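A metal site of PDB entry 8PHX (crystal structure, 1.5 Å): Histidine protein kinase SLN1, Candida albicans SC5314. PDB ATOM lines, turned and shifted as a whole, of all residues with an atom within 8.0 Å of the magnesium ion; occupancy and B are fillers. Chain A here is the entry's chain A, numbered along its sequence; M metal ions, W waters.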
ATOM      1  N   ALA A  13      -3.903 -13.256  31.407  1.00  0.00           N
ATOM      2  CA  ALA A  13      -4.059 -11.852  31.078  1.00  0.00           C
ATOM      3  C   ALA A  13      -3.437 -11.641  29.704  1.00  0.00           C
ATOM      4  O   ALA A  13      -2.245 -11.879  29.529  1.00  0.00           O
ATOM      5  CB  ALA A  13      -3.429 -10.962  32.102  1.00  0.00           C
ATOM      6  N   GLU A  14      -4.258 -11.200  28.755  1.00  0.00           N
ATOM      7  CA  GLU A  14      -3.846 -10.966  27.386  1.00  0.00           C
ATOM      8  C   GLU A  14      -4.820  -9.956  26.787  1.00  0.00           C
ATOM      9  O   GLU A  14      -6.023 -10.223  26.796  1.00  0.00           O
ATOM     10  CB  GLU A  14      -3.925 -12.270  26.619  1.00  0.00           C
ATOM     11  CG  GLU A  14      -2.628 -12.680  25.976  1.00  0.00           C
ATOM     12  CD  GLU A  14      -2.161 -11.882  24.772  1.00  0.00           C
ATOM     13  OE1 GLU A  14      -1.262 -12.415  24.114  1.00  0.00           O
ATOM     14  OE2 GLU A  14      -2.601 -10.712  24.522  1.00  0.00           O
ATOM     15  N   ASP A  15      -4.287  -8.854  26.251  1.00  0.00           N
ATOM     16  CA  ASP A  15      -5.174  -7.818  25.647  1.00  0.00           C
ATOM     17  C   ASP A  15      -5.505  -8.150  24.188  1.00  0.00           C
ATOM     18  O   ASP A  15      -6.315  -7.437  23.617  1.00  0.00           O
ATOM     19  CB  ASP A  15      -4.553  -6.439  25.803  1.00  0.00           C
ATOM     20  CG  ASP A  15      -3.193  -6.266  25.151  1.00  0.00           C
ATOM     21  OD1 ASP A  15      -2.354  -7.138  25.336  1.00  0.00           O
ATOM     22  OD2 ASP A  15      -3.009  -5.250  24.472  1.00  0.00           O
ATOM     23  N   ASN A  16      -4.897  -9.190  23.616  1.00  0.00           N
ATOM     24  CA  ASN A  16      -5.205  -9.645  22.236  1.00  0.00           C
ATOM     25  C   ASN A  16      -6.207 -10.801  22.326  1.00  0.00           C
ATOM     26  O   ASN A  16      -5.857 -11.851  22.804  1.00  0.00           O
ATOM     27  CB  ASN A  16      -3.922  -9.979  21.474  1.00  0.00           C
ATOM     28  CG  ASN A  16      -4.138 -10.381  20.037  1.00  0.00           C
ATOM     29  OD1 ASN A  16      -4.952 -11.243  19.738  1.00  0.00           O
ATOM     30  ND2 ASN A  16      -3.385  -9.784  19.145  1.00  0.00           N
ATOM     31  N   ASN A  19      -5.296 -14.019  20.545  1.00  0.00           N
ATOM     32  CA  ASN A  19      -4.350 -14.758  21.440  1.00  0.00           C
ATOM     33  C   ASN A  19      -4.993 -15.509  22.643  1.00  0.00           C
ATOM     34  O   ASN A  19      -4.718 -16.723  23.175  1.00  0.00           O
ATOM     35  CB  ASN A  19      -3.230 -13.843  21.953  1.00  0.00           C
ATOM     36  CG  ASN A  19      -2.296 -13.306  20.892  1.00  0.00           C
ATOM     37  OD1 ASN A  19      -1.400 -12.513  21.182  1.00  0.00           O
ATOM     38  ND2 ASN A  19      -2.478 -13.732  19.658  1.00  0.00           N
ATOM     39  N   CYS A  39      -8.406  -8.900  30.253  1.00  0.00           N
ATOM     40  CA  CYS A  39      -8.020  -8.110  29.045  1.00  0.00           C
ATOM     41  C   CYS A  39      -6.922  -7.091  29.358  1.00  0.00           C
ATOM     42  O   CYS A  39      -6.349  -6.583  28.426  1.00  0.00           O
ATOM     43  CB  CYS A  39      -9.235  -7.373  28.511  1.00  0.00           C
ATOM     44  SG  CYS A  39     -10.435  -8.458  27.699  1.00  0.00           S
ATOM     45  N   MET A  63       0.827 -13.931  32.223  1.00  0.00           N
ATOM     46  CA  MET A  63       0.666 -12.484  32.248  1.00  0.00           C
ATOM     47  C   MET A  63       1.329 -11.879  31.018  1.00  0.00           C
ATOM     48  O   MET A  63       2.554 -11.770  30.941  1.00  0.00           O
ATOM     49  CB  MET A  63       1.329 -11.905  33.500  1.00  0.00           C
ATOM     50  CG  MET A  63       1.191 -10.414  33.636  1.00  0.00           C
ATOM     51  SD  MET A  63      -0.451  -9.892  34.160  1.00  0.00           S
ATOM     52  CE  MET A  63      -0.435 -10.357  35.884  1.00  0.00           C
ATOM     53  N   ASP A  64       0.528 -11.389  30.082  1.00  0.00           N
ATOM     54  CA  ASP A  64       1.073 -10.641  28.963  1.00  0.00           C
ATOM     55  C   ASP A  64       1.795  -9.408  29.506  1.00  0.00           C
ATOM     56  O   ASP A  64       1.256  -8.692  30.361  1.00  0.00           O
ATOM     57  CB  ASP A  64      -0.042 -10.230  28.018  1.00  0.00           C
ATOM     58  CG  ASP A  64       0.481  -9.614  26.734  1.00  0.00           C
ATOM     59  OD1 ASP A  64       1.517 -10.082  26.227  1.00  0.00           O
ATOM     60  OD2 ASP A  64      -0.186  -8.700  26.246  1.00  0.00           O
ATOM     61  N   VAL A  65       2.992  -9.097  28.980  1.00  0.00           N
ATOM     62  CA  VAL A  65       3.728  -7.981  29.526  1.00  0.00           C
ATOM     63  C   VAL A  65       3.109  -6.641  29.094  1.00  0.00           C
ATOM     64  O   VAL A  65       3.001  -5.748  29.928  1.00  0.00           O
ATOM     65  CB  VAL A  65       5.212  -8.072  29.158  1.00  0.00           C
ATOM     66  CG1 VAL A  65       5.978  -6.826  29.550  1.00  0.00           C
ATOM     67  CG2 VAL A  65       5.819  -9.294  29.802  1.00  0.00           C
ATOM     68  N   GLN A  66       2.726  -6.521  27.828  1.00  0.00           N
ATOM     69  CA  GLN A  66       2.267  -5.246  27.297  1.00  0.00           C
ATOM     70  C   GLN A  66       0.751  -5.259  27.099  1.00  0.00           C
ATOM     71  O   GLN A  66       0.219  -5.920  26.214  1.00  0.00           O
ATOM     72  CB  GLN A  66       3.050  -4.915  26.034  1.00  0.00           C
ATOM     73  CG  GLN A  66       4.538  -4.779  26.318  1.00  0.00           C
ATOM     74  CD  GLN A  66       5.368  -4.226  25.185  1.00  0.00           C
ATOM     75  OE1 GLN A  66       5.036  -4.388  24.018  1.00  0.00           O
ATOM     76  NE2 GLN A  66       6.497  -3.633  25.535  1.00  0.00           N
ATOM     77  N   MET A  67       0.082  -4.486  27.946  1.00  0.00           N
ATOM     78  CA  MET A  67      -1.349  -4.344  27.916  1.00  0.00           C
ATOM     79  C   MET A  67      -1.690  -2.886  28.211  1.00  0.00           C
ATOM     80  O   MET A  67      -0.921  -2.201  28.890  1.00  0.00           O
ATOM     81  CB  MET A  67      -2.012  -5.221  28.986  1.00  0.00           C
ATOM     82  CG  MET A  67      -1.739  -6.728  28.810  1.00  0.00           C
ATOM     83  SD  MET A  67      -2.591  -7.769  30.038  1.00  0.00           S
ATOM     84  CE  MET A  67      -1.625  -7.415  31.502  1.00  0.00           C
ATOM     85  N   PRO A  68      -2.858  -2.405  27.758  1.00  0.00           N
ATOM     86  CA  PRO A  68      -3.234  -1.004  28.019  1.00  0.00           C
ATOM     87  C   PRO A  68      -3.765  -0.865  29.434  1.00  0.00           C
ATOM     88  O   PRO A  68      -4.124  -1.853  30.076  1.00  0.00           O
ATOM     89  CB  PRO A  68      -4.303  -0.759  26.957  1.00  0.00           C
ATOM     90  CG  PRO A  68      -4.975  -2.114  26.762  1.00  0.00           C
ATOM     91  CD  PRO A  68      -3.907  -3.144  27.063  1.00  0.00           C
ATOM     92  N   GLY A  72       1.469  -5.571  32.306  1.00  0.00           N
ATOM     93  CA  GLY A  72       1.785  -6.777  33.059  1.00  0.00           C
ATOM     94  C   GLY A  72       2.801  -6.578  34.174  1.00  0.00           C
ATOM     95  O   GLY A  72       2.789  -7.276  35.184  1.00  0.00           O
ATOM     96  N   LEU A  92       4.259 -13.445  29.215  1.00  0.00           N
ATOM     97  CA  LEU A  92       4.166 -13.661  27.783  1.00  0.00           C
ATOM     98  C   LEU A  92       4.766 -12.419  27.146  1.00  0.00           C
ATOM     99  O   LEU A  92       4.255 -11.322  27.351  1.00  0.00           O
ATOM    100  CB  LEU A  92       2.714 -13.882  27.356  1.00  0.00           C
ATOM    101  CG  LEU A  92       1.920 -14.930  28.126  1.00  0.00           C
ATOM    102  CD1 LEU A  92       0.464 -14.954  27.676  1.00  0.00           C
ATOM    103  CD2 LEU A  92       2.550 -16.293  27.967  1.00  0.00           C
ATOM    104  N   ALA A  94       6.671 -10.533  23.619  1.00  0.00           N
ATOM    105  CA  ALA A  94       6.903 -10.542  22.181  1.00  0.00           C
ATOM    106  C   ALA A  94       8.379 -10.383  21.888  1.00  0.00           C
ATOM    107  O   ALA A  94       8.808 -10.664  20.770  1.00  0.00           O
ATOM    108  CB  ALA A  94       6.130  -9.447  21.475  1.00  0.00           C
ATOM    109  N   LYS A 115       6.340 -15.041  22.674  1.00  0.00           N
ATOM    110  CA  LYS A 115       5.220 -15.224  21.784  1.00  0.00           C
ATOM    111  C   LYS A 115       5.772 -15.369  20.366  1.00  0.00           C
ATOM    112  O   LYS A 115       6.773 -14.764  20.032  1.00  0.00           O
ATOM    113  CB  LYS A 115       4.284 -14.009  21.894  1.00  0.00           C
ATOM    114  CG  LYS A 115       3.867 -13.728  23.337  1.00  0.00           C
ATOM    115  CD  LYS A 115       3.226 -12.372  23.605  1.00  0.00           C
ATOM    116  CE  LYS A 115       1.731 -12.471  23.536  1.00  0.00           C
ATOM    117  NZ  LYS A 115       1.104 -11.127  23.683  1.00  0.00           N
HETATM  118 MG    MG M   1      -0.345  -7.329  24.791  1.00  0.00          MG
HETATM  119  O   HOH W   1      -0.621  -5.804  23.406  1.00  0.00           O
HETATM  120  O   HOH W   2       1.600  -7.493  23.999  1.00  0.00           O
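The magnesium ion is bound by the side-chain carboxylate of Asp 64 (2.0 Å), water W1 (2.1 Å), the backbone carbonyl oxygen of Gln 66 (2.1 Å), the side-chain carboxylate of Asp 15 (2.1 Å) and water W2 (2.1 Å). The magnesium ion has five donor atoms within binding distance.
The side-chain carboxylate (OD1) of Asp 64 is in salt-bridge range of the side-chain amino group (NZ) of Lys 115 (2.8 Å). N of Asp 64 sits at hydrogen-bond distance from O of Ala 13, at 2.9 Å.
The nearest printed residue that does not touch the magnesium ion is Glu 14 (4.1 Å).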
